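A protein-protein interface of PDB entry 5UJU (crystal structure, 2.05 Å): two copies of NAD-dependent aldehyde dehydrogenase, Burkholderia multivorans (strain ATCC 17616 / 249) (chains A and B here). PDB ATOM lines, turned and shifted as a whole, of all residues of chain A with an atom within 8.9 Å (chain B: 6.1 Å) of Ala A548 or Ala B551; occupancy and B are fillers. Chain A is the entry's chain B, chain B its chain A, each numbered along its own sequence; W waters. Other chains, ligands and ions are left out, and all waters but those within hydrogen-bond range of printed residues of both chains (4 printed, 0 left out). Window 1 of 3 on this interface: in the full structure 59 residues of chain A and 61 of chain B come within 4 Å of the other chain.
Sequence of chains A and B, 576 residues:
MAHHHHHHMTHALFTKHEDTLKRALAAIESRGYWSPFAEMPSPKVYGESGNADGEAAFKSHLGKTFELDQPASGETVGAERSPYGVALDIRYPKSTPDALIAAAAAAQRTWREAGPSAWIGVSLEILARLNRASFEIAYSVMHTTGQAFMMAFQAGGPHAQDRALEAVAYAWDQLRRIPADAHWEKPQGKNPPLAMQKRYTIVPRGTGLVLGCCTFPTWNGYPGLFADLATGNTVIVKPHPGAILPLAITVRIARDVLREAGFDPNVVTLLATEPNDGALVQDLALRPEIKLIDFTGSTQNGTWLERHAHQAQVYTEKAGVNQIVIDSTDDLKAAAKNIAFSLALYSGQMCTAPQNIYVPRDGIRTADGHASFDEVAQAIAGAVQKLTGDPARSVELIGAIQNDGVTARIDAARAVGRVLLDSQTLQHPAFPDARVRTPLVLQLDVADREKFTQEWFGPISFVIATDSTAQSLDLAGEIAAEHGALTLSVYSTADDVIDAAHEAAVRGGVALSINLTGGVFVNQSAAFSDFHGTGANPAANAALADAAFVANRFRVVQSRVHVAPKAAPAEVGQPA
NE2 of Gln B174 sits at hydrogen-bond distance from OE1 of Gln A174 (3.4 Å).
The guanidinium group (NH1) of Arg B555 sits at hydrogen-bond distance from the backbone carbonyl oxygen (O) of Thr A534 (2.8 Å).
The guanidinium group (NH2) of Arg B555 lies within salt-bridge range of the side-chain carboxylate (OD2) of Asp A546, at 2.8 Å.
OD1 of Asp B546 sits close to N of Ala B548 (3.3 Å).
The backbone carbonyl oxygen (O) of Ala B551 lies within hydrogen-bond range of the guanidinium group (NH2) of Arg B555, at 3.2 Å.
NE2 of Gln A313 lies within hydrogen-bond range of O of Asn A552.
The backbone NH (N) of Ala A548 lies close to the side-chain carboxylate (OD1) of Asp A546 (3.3 Å).
OD1 of Asp A546 lies within hydrogen-bond range of N of Phe A549.
Among the printed residues, pairs that only touch across the chains: Gln A174 with Ala B547 (3.6 Å), Gly A535 with Arg B555 (3.98 Å), Ala A543 with Arg B555 (3.9 Å), Ala A547 with Gln B174 (3.0 Å), Ala A547 with Ala B551 (3.9 Å), Ala A548 with Ala B551 (3.6 Å), Ala A548 with Asn B552 (3.6 Å), Ala A548 with Arg B555 (3.6 Å), Ala A551 with Ala B547 (3.99 Å), Ala A551 with Ala B548 (3.7 Å) and Asn A552 with Ala B548 (3.6 Å).
Printed residues of chain B within 4 Å of Ala A543: Arg B555.
Ala A548 touches three residues of chain B.
Of the printed residues of chain B, Asn A552 touches Ala B548.
Of the printed residues of chain A, Ala B547 touches Gln A174 (3.6 Å) and Ala A551 (3.99 Å).
No residue of chain A comes within 4 Å of Val B550.
Ala B551 touches just these residues of chain A: Ala A547 (3.9 Å) and Ala A548 (3.6 Å).
Asn B552 touches just one residue of chain A: Ala A548 (3.6 Å).
Phe B554 touches none of the printed residues of chain A.
The nearest residue of chain B that does not touch Ala A548 is Gln B174 (5.9 Å).
Hydrophobic or aromatic side chains of chain B that line the printed part of chain A: Ala B547, Ala B548 and Ala B551.
Along chain B the printed residues that touch a printed residue of chain A span positions 174 to 555.
Of the 24 printed residues of chain A, 9 touch a printed residue of chain B.
Hydrophobic or aromatic side chains of chain A within 4 Å of the printed part of chain B: Ala A543, Ala A547, Ala A548 and Ala A551.
Gln A174 touches its own counterpart, Gln B174.
Gln A174 touches Ala B547, and with the chains exchanged Ala A547 touches Gln B174.
Ala A547 touches Ala B551, and with the chains exchanged Ala A551 touches Ala B547.
Ala A548 touches Ala B551, and with the chains exchanged Ala A551 touches Ala B548.
Of the 14 pairs that touch across the chains among the printed residues, 9 have their exchanged pair printed and touching as well.
Water W2 lies within hydrogen-bond range of OD1 of Asp A546 (2.6 Å), N of Ala A543 (2.8 Å) and NH1 of Arg B555 (3.3 Å).
Water W3 bridges the side-chain amide oxygen (OD1) of Asn B552 (2.8 Å) and the backbone carbonyl oxygen (O) of Asn A541 (3.3 Å).
Water W1 lies within hydrogen-bond range of the backbone carbonyl oxygen (O) of Ala B551, the guanidinium group (NH2) of Arg B555, the backbone NH (N) of Ala A548 and the side-chain carboxylate (OD2) of Asp A546.
Water W4 lies within hydrogen-bond range of the backbone carbonyl oxygen of Ala A551, the backbone NH of Ala B548 and the side-chain carboxylate of Asp B546.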
ATOM      1  N   TYR A 170     -16.862 -22.831 -15.823  1.00  0.00           N
ATOM      2  CA  TYR A 170     -16.613 -23.207 -17.209  1.00  0.00           C
ATOM      3  C   TYR A 170     -16.815 -22.018 -18.145  1.00  0.00           C
ATOM      4  O   TYR A 170     -16.016 -21.794 -19.060  1.00  0.00           O
ATOM      5  CB  TYR A 170     -17.514 -24.379 -17.612  1.00  0.00           C
ATOM      6  CG  TYR A 170     -16.903 -25.733 -17.267  1.00  0.00           C
ATOM      7  CD1 TYR A 170     -15.917 -26.292 -18.077  1.00  0.00           C
ATOM      8  CD2 TYR A 170     -17.310 -26.450 -16.129  1.00  0.00           C
ATOM      9  CE1 TYR A 170     -15.348 -27.537 -17.766  1.00  0.00           C
ATOM     10  CE2 TYR A 170     -16.745 -27.693 -15.809  1.00  0.00           C
ATOM     11  CZ  TYR A 170     -15.763 -28.221 -16.637  1.00  0.00           C
ATOM     12  OH  TYR A 170     -15.196 -29.435 -16.359  1.00  0.00           O
ATOM     13  N   ALA A 171     -17.871 -21.236 -17.925  1.00  0.00           N
ATOM     14  CA  ALA A 171     -18.043 -20.029 -18.729  1.00  0.00           C
ATOM     15  C   ALA A 171     -16.811 -19.138 -18.626  1.00  0.00           C
ATOM     16  O   ALA A 171     -16.177 -18.812 -19.636  1.00  0.00           O
ATOM     17  CB  ALA A 171     -19.299 -19.275 -18.283  1.00  0.00           C
ATOM     18  N   GLN A 174     -13.649 -20.132 -20.448  1.00  0.00           N
ATOM     19  CA  GLN A 174     -13.609 -19.819 -21.875  1.00  0.00           C
ATOM     20  C   GLN A 174     -13.383 -18.322 -22.092  1.00  0.00           C
ATOM     21  O   GLN A 174     -12.531 -17.923 -22.894  1.00  0.00           O
ATOM     22  CB  GLN A 174     -14.920 -20.231 -22.557  1.00  0.00           C
ATOM     23  CG  GLN A 174     -15.382 -21.644 -22.233  1.00  0.00           C
ATOM     24  CD  GLN A 174     -14.330 -22.718 -22.472  1.00  0.00           C
ATOM     25  OE1 GLN A 174     -13.560 -22.663 -23.433  1.00  0.00           O
ATOM     26  NE2 GLN A 174     -14.253 -23.668 -21.536  1.00  0.00           N
ATOM     27  N   ALA A 227     -25.270 -20.805 -16.811  1.00  0.00           N
ATOM     28  CA  ALA A 227     -24.478 -20.760 -18.035  1.00  0.00           C
ATOM     29  C   ALA A 227     -24.936 -19.606 -18.929  1.00  0.00           C
ATOM     30  O   ALA A 227     -24.110 -18.892 -19.514  1.00  0.00           O
ATOM     31  CB  ALA A 227     -24.576 -22.090 -18.785  1.00  0.00           C
ATOM     32  N   ASP A 294     -32.393 -24.524 -22.718  1.00  0.00           N
ATOM     33  CA  ASP A 294     -31.963 -25.608 -21.839  1.00  0.00           C
ATOM     34  C   ASP A 294     -33.217 -26.304 -21.331  1.00  0.00           C
ATOM     35  O   ASP A 294     -34.074 -25.667 -20.703  1.00  0.00           O
ATOM     36  CB  ASP A 294     -31.119 -25.079 -20.680  1.00  0.00           C
ATOM     37  CG  ASP A 294     -29.726 -24.652 -21.125  1.00  0.00           C
ATOM     38  OD1 ASP A 294     -28.773 -25.457 -20.972  1.00  0.00           O
ATOM     39  OD2 ASP A 294     -29.591 -23.516 -21.641  1.00  0.00           O
ATOM     40  N   GLN A 313     -29.673 -22.744 -29.986  1.00  0.00           N
ATOM     41  CA  GLN A 313     -28.853 -23.831 -29.476  1.00  0.00           C
ATOM     42  C   GLN A 313     -29.656 -24.532 -28.401  1.00  0.00           C
ATOM     43  O   GLN A 313     -30.039 -23.904 -27.408  1.00  0.00           O
ATOM     44  CB  GLN A 313     -27.554 -23.319 -28.871  1.00  0.00           C
ATOM     45  CG  GLN A 313     -26.574 -22.692 -29.796  1.00  0.00           C
ATOM     46  CD  GLN A 313     -25.617 -21.816 -29.029  1.00  0.00           C
ATOM     47  OE1 GLN A 313     -25.325 -22.071 -27.857  1.00  0.00           O
ATOM     48  NE2 GLN A 313     -25.085 -20.810 -29.687  1.00  0.00           N
ATOM     49  N   VAL A 314     -29.917 -25.824 -28.588  1.00  0.00           N
ATOM     50  CA  VAL A 314     -30.792 -26.568 -27.697  1.00  0.00           C
ATOM     51  C   VAL A 314     -29.943 -27.550 -26.904  1.00  0.00           C
ATOM     52  O   VAL A 314     -29.241 -28.392 -27.484  1.00  0.00           O
ATOM     53  CB  VAL A 314     -31.907 -27.277 -28.473  1.00  0.00           C
ATOM     54  CG1 VAL A 314     -32.845 -27.977 -27.510  1.00  0.00           C
ATOM     55  CG2 VAL A 314     -32.668 -26.258 -29.328  1.00  0.00           C
ATOM     56  N   TYR A 315     -30.019 -27.448 -25.579  1.00  0.00           N
ATOM     57  CA  TYR A 315     -29.349 -28.360 -24.657  1.00  0.00           C
ATOM     58  C   TYR A 315     -30.422 -29.130 -23.914  1.00  0.00           C
ATOM     59  O   TYR A 315     -31.336 -28.523 -23.353  1.00  0.00           O
ATOM     60  CB  TYR A 315     -28.459 -27.606 -23.661  1.00  0.00           C
ATOM     61  CG  TYR A 315     -27.487 -26.656 -24.315  1.00  0.00           C
ATOM     62  CD1 TYR A 315     -26.213 -27.079 -24.663  1.00  0.00           C
ATOM     63  CD2 TYR A 315     -27.841 -25.336 -24.578  1.00  0.00           C
ATOM     64  CE1 TYR A 315     -25.317 -26.222 -25.265  1.00  0.00           C
ATOM     65  CE2 TYR A 315     -26.954 -24.474 -25.184  1.00  0.00           C
ATOM     66  CZ  TYR A 315     -25.695 -24.924 -25.525  1.00  0.00           C
ATOM     67  OH  TYR A 315     -24.786 -24.084 -26.123  1.00  0.00           O
ATOM     68  N   PHE A 531     -18.876 -35.669 -14.385  1.00  0.00           N
ATOM     69  CA  PHE A 531     -19.725 -35.212 -15.474  1.00  0.00           C
ATOM     70  C   PHE A 531     -21.091 -35.878 -15.349  1.00  0.00           C
ATOM     71  O   PHE A 531     -21.181 -37.108 -15.246  1.00  0.00           O
ATOM     72  CB  PHE A 531     -19.090 -35.542 -16.821  1.00  0.00           C
ATOM     73  CG  PHE A 531     -17.780 -34.865 -17.045  1.00  0.00           C
ATOM     74  CD1 PHE A 531     -17.730 -33.506 -17.339  1.00  0.00           C
ATOM     75  CD2 PHE A 531     -16.604 -35.579 -16.991  1.00  0.00           C
ATOM     76  CE1 PHE A 531     -16.509 -32.867 -17.544  1.00  0.00           C
ATOM     77  CE2 PHE A 531     -15.385 -34.962 -17.205  1.00  0.00           C
ATOM     78  CZ  PHE A 531     -15.330 -33.598 -17.483  1.00  0.00           C
ATOM     79  N   THR A 534     -22.991 -37.602 -20.561  1.00  0.00           N
ATOM     80  CA  THR A 534     -21.840 -37.348 -21.419  1.00  0.00           C
ATOM     81  C   THR A 534     -22.167 -36.434 -22.587  1.00  0.00           C
ATOM     82  O   THR A 534     -21.273 -35.752 -23.099  1.00  0.00           O
ATOM     83  CB  THR A 534     -21.290 -38.659 -21.988  1.00  0.00           C
ATOM     84  OG1 THR A 534     -22.284 -39.250 -22.838  1.00  0.00           O
ATOM     85  CG2 THR A 534     -20.922 -39.639 -20.860  1.00  0.00           C
ATOM     86  N   GLY A 535     -23.421 -36.424 -23.027  1.00  0.00           N
ATOM     87  CA  GLY A 535     -23.765 -35.827 -24.290  1.00  0.00           C
ATOM     88  C   GLY A 535     -23.567 -36.734 -25.480  1.00  0.00           C
ATOM     89  O   GLY A 535     -23.771 -36.295 -26.615  1.00  0.00           O
ATOM     90  N   ASN A 541     -27.997 -34.399 -24.809  1.00  0.00           N
ATOM     91  CA  ASN A 541     -27.094 -33.984 -25.871  1.00  0.00           C
ATOM     92  C   ASN A 541     -25.977 -33.082 -25.368  1.00  0.00           C
ATOM     93  O   ASN A 541     -25.249 -32.502 -26.177  1.00  0.00           O
ATOM     94  CB  ASN A 541     -27.880 -33.323 -27.005  1.00  0.00           C
ATOM     95  CG  ASN A 541     -28.334 -31.905 -26.673  1.00  0.00           C
ATOM     96  OD1 ASN A 541     -28.142 -31.408 -25.563  1.00  0.00           O
ATOM     97  ND2 ASN A 541     -28.981 -31.269 -27.636  1.00  0.00           N
ATOM     98  N   ALA A 542     -25.837 -32.947 -24.051  1.00  0.00           N
ATOM     99  CA  ALA A 542     -24.786 -32.140 -23.445  1.00  0.00           C
ATOM    100  C   ALA A 542     -24.417 -32.764 -22.106  1.00  0.00           C
ATOM    101  O   ALA A 542     -25.209 -33.496 -21.504  1.00  0.00           O
ATOM    102  CB  ALA A 542     -25.226 -30.682 -23.250  1.00  0.00           C
ATOM    103  N   ALA A 543     -23.216 -32.445 -21.632  1.00  0.00           N
ATOM    104  CA  ALA A 543     -22.751 -32.870 -20.321  1.00  0.00           C
ATOM    105  C   ALA A 543     -22.803 -31.692 -19.351  1.00  0.00           C
ATOM    106  O   ALA A 543     -22.541 -30.553 -19.736  1.00  0.00           O
ATOM    107  CB  ALA A 543     -21.323 -33.423 -20.399  1.00  0.00           C
ATOM    108  N   LEU A 544     -23.153 -31.971 -18.095  1.00  0.00           N
ATOM    109  CA  LEU A 544     -23.094 -30.980 -17.014  1.00  0.00           C
ATOM    110  C   LEU A 544     -21.834 -31.239 -16.193  1.00  0.00           C
ATOM    111  O   LEU A 544     -21.789 -32.195 -15.418  1.00  0.00           O
ATOM    112  CB  LEU A 544     -24.330 -31.072 -16.123  1.00  0.00           C
ATOM    113  CG  LEU A 544     -25.690 -30.903 -16.794  1.00  0.00           C
ATOM    114  CD1 LEU A 544     -26.824 -31.089 -15.788  1.00  0.00           C
ATOM    115  CD2 LEU A 544     -25.766 -29.525 -17.433  1.00  0.00           C
ATOM    116  N   ALA A 545     -20.797 -30.417 -16.358  1.00  0.00           N
ATOM    117  CA  ALA A 545     -20.680 -29.376 -17.364  1.00  0.00           C
ATOM    118  C   ALA A 545     -19.286 -29.487 -17.965  1.00  0.00           C
ATOM    119  O   ALA A 545     -18.364 -29.997 -17.323  1.00  0.00           O
ATOM    120  CB  ALA A 545     -20.889 -27.987 -16.753  1.00  0.00           C
ATOM    121  N   ASP A 546     -19.118 -29.012 -19.194  1.00  0.00           N
ATOM    122  CA  ASP A 546     -17.812 -29.043 -19.839  1.00  0.00           C
ATOM    123  C   ASP A 546     -17.696 -27.805 -20.723  1.00  0.00           C
ATOM    124  O   ASP A 546     -18.562 -26.924 -20.699  1.00  0.00           O
ATOM    125  CB  ASP A 546     -17.606 -30.360 -20.608  1.00  0.00           C
ATOM    126  CG  ASP A 546     -18.651 -30.595 -21.698  1.00  0.00           C
ATOM    127  OD1 ASP A 546     -19.504 -29.704 -21.946  1.00  0.00           O
ATOM    128  OD2 ASP A 546     -18.620 -31.690 -22.310  1.00  0.00           O
ATOM    129  N   ALA A 547     -16.609 -27.728 -21.491  1.00  0.00           N
ATOM    130  CA  ALA A 547     -16.399 -26.573 -22.356  1.00  0.00           C
ATOM    131  C   ALA A 547     -17.527 -26.429 -23.373  1.00  0.00           C
ATOM    132  O   ALA A 547     -18.014 -25.313 -23.617  1.00  0.00           O
ATOM    133  CB  ALA A 547     -15.052 -26.694 -23.068  1.00  0.00           C
ATOM    134  N   ALA A 548     -17.949 -27.549 -23.980  1.00  0.00           N
ATOM    135  CA  ALA A 548     -18.996 -27.513 -24.996  1.00  0.00           C
ATOM    136  C   ALA A 548     -20.323 -27.026 -24.433  1.00  0.00           C
ATOM    137  O   ALA A 548     -21.156 -26.521 -25.190  1.00  0.00           O
ATOM    138  CB  ALA A 548     -19.179 -28.901 -25.636  1.00  0.00           C
ATOM    139  N   PHE A 549     -20.543 -27.183 -23.126  1.00  0.00           N
ATOM    140  CA  PHE A 549     -21.787 -26.731 -22.516  1.00  0.00           C
ATOM    141  C   PHE A 549     -21.918 -25.202 -22.480  1.00  0.00           C
ATOM    142  O   PHE A 549     -23.041 -24.704 -22.359  1.00  0.00           O
ATOM    143  CB  PHE A 549     -21.888 -27.295 -21.098  1.00  0.00           C
ATOM    144  CG  PHE A 549     -23.203 -27.019 -20.419  1.00  0.00           C
ATOM    145  CD1 PHE A 549     -24.370 -27.603 -20.878  1.00  0.00           C
ATOM    146  CD2 PHE A 549     -23.261 -26.191 -19.305  1.00  0.00           C
ATOM    147  CE1 PHE A 549     -25.575 -27.364 -20.245  1.00  0.00           C
ATOM    148  CE2 PHE A 549     -24.464 -25.941 -18.671  1.00  0.00           C
ATOM    149  CZ  PHE A 549     -25.622 -26.534 -19.143  1.00  0.00           C
ATOM    150  N   VAL A 550     -20.813 -24.461 -22.568  1.00  0.00           N
ATOM    151  CA  VAL A 550     -20.846 -23.004 -22.445  1.00  0.00           C
ATOM    152  C   VAL A 550     -20.228 -22.270 -23.634  1.00  0.00           C
ATOM    153  O   VAL A 550     -20.566 -21.092 -23.859  1.00  0.00           O
ATOM    154  CB  VAL A 550     -20.162 -22.537 -21.141  1.00  0.00           C
ATOM    155  CG1 VAL A 550     -20.879 -23.079 -19.914  1.00  0.00           C
ATOM    156  CG2 VAL A 550     -18.695 -22.968 -21.135  1.00  0.00           C
ATOM    157  N   ALA A 551     -19.337 -22.892 -24.405  1.00  0.00           N
ATOM    158  CA  ALA A 551     -18.501 -22.150 -25.339  1.00  0.00           C
ATOM    159  C   ALA A 551     -19.276 -21.528 -26.500  1.00  0.00           C
ATOM    160  O   ALA A 551     -18.731 -20.654 -27.174  1.00  0.00           O
ATOM    161  CB  ALA A 551     -17.410 -23.059 -25.906  1.00  0.00           C
ATOM    162  N   ASN A 552     -20.494 -21.992 -26.777  1.00  0.00           N
ATOM    163  CA  ASN A 552     -21.303 -21.517 -27.888  1.00  0.00           C
ATOM    164  C   ASN A 552     -22.332 -20.466 -27.482  1.00  0.00           C
ATOM    165  O   ASN A 552     -23.026 -19.940 -28.359  1.00  0.00           O
ATOM    166  CB  ASN A 552     -22.022 -22.692 -28.563  1.00  0.00           C
ATOM    167  CG  ASN A 552     -22.043 -22.577 -30.085  1.00  0.00           C
ATOM    168  OD1 ASN A 552     -21.417 -21.688 -30.672  1.00  0.00           O
ATOM    169  ND2 ASN A 552     -22.748 -23.492 -30.730  1.00  0.00           N
ATOM    170  N   ARG A 553     -22.441 -20.138 -26.189  1.00  0.00           N
ATOM    171  CA  ARG A 553     -23.460 -19.211 -25.688  1.00  0.00           C
ATOM    172  C   ARG A 553     -23.062 -17.752 -25.836  1.00  0.00           C
ATOM    173  O   ARG A 553     -23.851 -16.869 -25.470  1.00  0.00           O
ATOM    174  CB  ARG A 553     -23.767 -19.504 -24.222  1.00  0.00           C
ATOM    175  CG  ARG A 553     -24.176 -20.962 -23.985  1.00  0.00           C
ATOM    176  CD  ARG A 553     -24.605 -21.228 -22.536  1.00  0.00           C
ATOM    177  NE  ARG A 553     -24.871 -22.654 -22.293  1.00  0.00           N
ATOM    178  CZ  ARG A 553     -26.076 -23.178 -22.062  1.00  0.00           C
ATOM    179  NH1 ARG A 553     -27.160 -22.397 -22.013  1.00  0.00           N
ATOM    180  NH2 ARG A 553     -26.197 -24.487 -21.856  1.00  0.00           N
ATOM    181  N   GLN B 174      -8.445 -27.633 -25.445  1.00  0.00           N
ATOM    182  CA  GLN B 174      -9.505 -28.272 -24.665  1.00  0.00           C
ATOM    183  C   GLN B 174      -9.062 -29.618 -24.087  1.00  0.00           C
ATOM    184  O   GLN B 174      -9.379 -29.940 -22.937  1.00  0.00           O
ATOM    185  CB  GLN B 174     -10.750 -28.496 -25.528  1.00  0.00           C
ATOM    186  CG  GLN B 174     -11.413 -27.259 -26.052  1.00  0.00           C
ATOM    187  CD  GLN B 174     -11.789 -26.340 -24.915  1.00  0.00           C
ATOM    188  OE1 GLN B 174     -12.117 -26.799 -23.816  1.00  0.00           O
ATOM    189  NE2 GLN B 174     -11.775 -25.049 -25.166  1.00  0.00           N
ATOM    190  N   TYR B 315     -21.296 -27.983 -38.830  1.00  0.00           N
ATOM    191  CA  TYR B 315     -20.591 -26.709 -38.902  1.00  0.00           C
ATOM    192  C   TYR B 315     -20.642 -26.224 -40.339  1.00  0.00           C
ATOM    193  O   TYR B 315     -20.251 -26.956 -41.250  1.00  0.00           O
ATOM    194  CB  TYR B 315     -19.144 -26.861 -38.445  1.00  0.00           C
ATOM    195  CG  TYR B 315     -19.029 -27.559 -37.107  1.00  0.00           C
ATOM    196  CD1 TYR B 315     -19.029 -26.825 -35.925  1.00  0.00           C
ATOM    197  CD2 TYR B 315     -18.929 -28.945 -37.026  1.00  0.00           C
ATOM    198  CE1 TYR B 315     -18.929 -27.436 -34.699  1.00  0.00           C
ATOM    199  CE2 TYR B 315     -18.837 -29.581 -35.796  1.00  0.00           C
ATOM    200  CZ  TYR B 315     -18.842 -28.818 -34.634  1.00  0.00           C
ATOM    201  OH  TYR B 315     -18.739 -29.413 -33.403  1.00  0.00           O
ATOM    202  N   ASP B 546     -12.500 -21.294 -32.836  1.00  0.00           N
ATOM    203  CA  ASP B 546     -12.616 -20.964 -31.420  1.00  0.00           C
ATOM    204  C   ASP B 546     -12.924 -22.240 -30.641  1.00  0.00           C
ATOM    205  O   ASP B 546     -12.947 -23.345 -31.203  1.00  0.00           O
ATOM    206  CB  ASP B 546     -13.685 -19.886 -31.189  1.00  0.00           C
ATOM    207  CG  ASP B 546     -15.084 -20.321 -31.647  1.00  0.00           C
ATOM    208  OD1 ASP B 546     -15.286 -21.486 -32.066  1.00  0.00           O
ATOM    209  OD2 ASP B 546     -16.000 -19.485 -31.580  1.00  0.00           O
ATOM    210  N   ALA B 547     -13.182 -22.076 -29.339  1.00  0.00           N
ATOM    211  CA  ALA B 547     -13.452 -23.228 -28.482  1.00  0.00           C
ATOM    212  C   ALA B 547     -14.692 -23.980 -28.936  1.00  0.00           C
ATOM    213  O   ALA B 547     -14.703 -25.212 -28.946  1.00  0.00           O
ATOM    214  CB  ALA B 547     -13.591 -22.787 -27.025  1.00  0.00           C
ATOM    215  N   ALA B 548     -15.757 -23.260 -29.297  1.00  0.00           N
ATOM    216  CA  ALA B 548     -16.972 -23.940 -29.724  1.00  0.00           C
ATOM    217  C   ALA B 548     -16.730 -24.758 -30.984  1.00  0.00           C
ATOM    218  O   ALA B 548     -17.434 -25.740 -31.228  1.00  0.00           O
ATOM    219  CB  ALA B 548     -18.101 -22.932 -29.964  1.00  0.00           C
ATOM    220  N   PHE B 549     -15.729 -24.380 -31.782  1.00  0.00           N
ATOM    221  CA  PHE B 549     -15.463 -25.082 -33.027  1.00  0.00           C
ATOM    222  C   PHE B 549     -14.921 -26.497 -32.795  1.00  0.00           C
ATOM    223  O   PHE B 549     -15.037 -27.325 -33.706  1.00  0.00           O
ATOM    224  CB  PHE B 549     -14.488 -24.277 -33.898  1.00  0.00           C
ATOM    225  CG  PHE B 549     -14.302 -24.836 -35.293  1.00  0.00           C
ATOM    226  CD1 PHE B 549     -15.336 -24.784 -36.215  1.00  0.00           C
ATOM    227  CD2 PHE B 549     -13.103 -25.420 -35.671  1.00  0.00           C
ATOM    228  CE1 PHE B 549     -15.173 -25.295 -37.499  1.00  0.00           C
ATOM    229  CE2 PHE B 549     -12.925 -25.928 -36.948  1.00  0.00           C
ATOM    230  CZ  PHE B 549     -13.965 -25.867 -37.869  1.00  0.00           C
ATOM    231  N   VAL B 550     -14.361 -26.790 -31.620  1.00  0.00           N
ATOM    232  CA  VAL B 550     -13.754 -28.104 -31.349  1.00  0.00           C
ATOM    233  C   VAL B 550     -14.306 -28.803 -30.110  1.00  0.00           C
ATOM    234  O   VAL B 550     -14.205 -30.047 -30.013  1.00  0.00           O
ATOM    235  CB  VAL B 550     -12.219 -27.978 -31.219  1.00  0.00           C
ATOM    236  CG1 VAL B 550     -11.604 -27.411 -32.469  1.00  0.00           C
ATOM    237  CG2 VAL B 550     -11.844 -27.151 -29.986  1.00  0.00           C
ATOM    238  N   ALA B 551     -14.866 -28.097 -29.124  1.00  0.00           N
ATOM    239  CA  ALA B 551     -15.119 -28.688 -27.811  1.00  0.00           C
ATOM    240  C   ALA B 551     -16.175 -29.781 -27.836  1.00  0.00           C
ATOM    241  O   ALA B 551     -16.243 -30.576 -26.893  1.00  0.00           O
ATOM    242  CB  ALA B 551     -15.546 -27.613 -26.809  1.00  0.00           C
ATOM    243  N   ASN B 552     -17.010 -29.828 -28.863  1.00  0.00           N
ATOM    244  CA  ASN B 552     -18.049 -30.842 -28.954  1.00  0.00           C
ATOM    245  C   ASN B 552     -17.636 -32.045 -29.802  1.00  0.00           C
ATOM    246  O   ASN B 552     -18.447 -32.951 -29.986  1.00  0.00           O
ATOM    247  CB  ASN B 552     -19.330 -30.244 -29.537  1.00  0.00           C
ATOM    248  CG  ASN B 552     -20.572 -30.763 -28.860  1.00  0.00           C
ATOM    249  OD1 ASN B 552     -20.502 -31.472 -27.853  1.00  0.00           O
ATOM    250  ND2 ASN B 552     -21.727 -30.414 -29.408  1.00  0.00           N
ATOM    251  N   ARG B 553     -16.430 -32.053 -30.375  1.00  0.00           N
ATOM    252  CA  ARG B 553     -16.049 -33.144 -31.277  1.00  0.00           C
ATOM    253  C   ARG B 553     -15.508 -34.365 -30.546  1.00  0.00           C
ATOM    254  O   ARG B 553     -15.266 -35.398 -31.187  1.00  0.00           O
ATOM    255  CB  ARG B 553     -15.015 -32.651 -32.300  1.00  0.00           C
ATOM    256  CG  ARG B 553     -15.488 -31.400 -33.099  1.00  0.00           C
ATOM    257  CD  ARG B 553     -14.479 -31.027 -34.190  1.00  0.00           C
ATOM    258  NE  ARG B 553     -14.858 -29.784 -34.863  1.00  0.00           N
ATOM    259  CZ  ARG B 553     -15.321 -29.698 -36.109  1.00  0.00           C
ATOM    260  NH1 ARG B 553     -15.464 -30.785 -36.869  1.00  0.00           N
ATOM    261  NH2 ARG B 553     -15.648 -28.504 -36.600  1.00  0.00           N
ATOM    262  N   PHE B 554     -15.314 -34.272 -29.236  1.00  0.00           N
ATOM    263  CA  PHE B 554     -14.969 -35.409 -28.391  1.00  0.00           C
ATOM    264  C   PHE B 554     -15.893 -35.354 -27.188  1.00  0.00           C
ATOM    265  O   PHE B 554     -16.506 -34.314 -26.905  1.00  0.00           O
ATOM    266  CB  PHE B 554     -13.496 -35.366 -27.919  1.00  0.00           C
ATOM    267  CG  PHE B 554     -13.202 -34.187 -27.033  1.00  0.00           C
ATOM    268  CD1 PHE B 554     -13.273 -34.301 -25.648  1.00  0.00           C
ATOM    269  CD2 PHE B 554     -12.922 -32.945 -27.585  1.00  0.00           C
ATOM    270  CE1 PHE B 554     -13.039 -33.204 -24.829  1.00  0.00           C
ATOM    271  CE2 PHE B 554     -12.697 -31.841 -26.770  1.00  0.00           C
ATOM    272  CZ  PHE B 554     -12.752 -31.969 -25.394  1.00  0.00           C
ATOM    273  N   ARG B 555     -16.004 -36.483 -26.492  1.00  0.00           N
ATOM    274  CA  ARG B 555     -16.714 -36.550 -25.226  1.00  0.00           C
ATOM    275  C   ARG B 555     -15.790 -37.193 -24.199  1.00  0.00           C
ATOM    276  O   ARG B 555     -14.704 -37.679 -24.534  1.00  0.00           O
ATOM    277  CB  ARG B 555     -18.041 -37.315 -25.359  1.00  0.00           C
ATOM    278  CG  ARG B 555     -19.025 -36.775 -26.416  1.00  0.00           C
ATOM    279  CD  ARG B 555     -19.806 -35.525 -25.949  1.00  0.00           C
ATOM    280  NE  ARG B 555     -18.947 -34.344 -25.888  1.00  0.00           N
ATOM    281  CZ  ARG B 555     -19.091 -33.351 -25.019  1.00  0.00           C
ATOM    282  NH1 ARG B 555     -20.070 -33.387 -24.129  1.00  0.00           N
ATOM    283  NH2 ARG B 555     -18.239 -32.328 -25.029  1.00  0.00           N
HETATM  284  O   HOH W   1     -16.368 -30.151 -24.062  1.00  0.00           O
HETATM  285  O   HOH W   2     -21.629 -30.640 -23.163  1.00  0.00           O
HETATM  286  O   HOH W   3     -22.350 -30.969 -25.833  1.00  0.00           O
HETATM  287  O   HOH W   4     -16.060 -20.351 -28.239  1.00  0.00           O
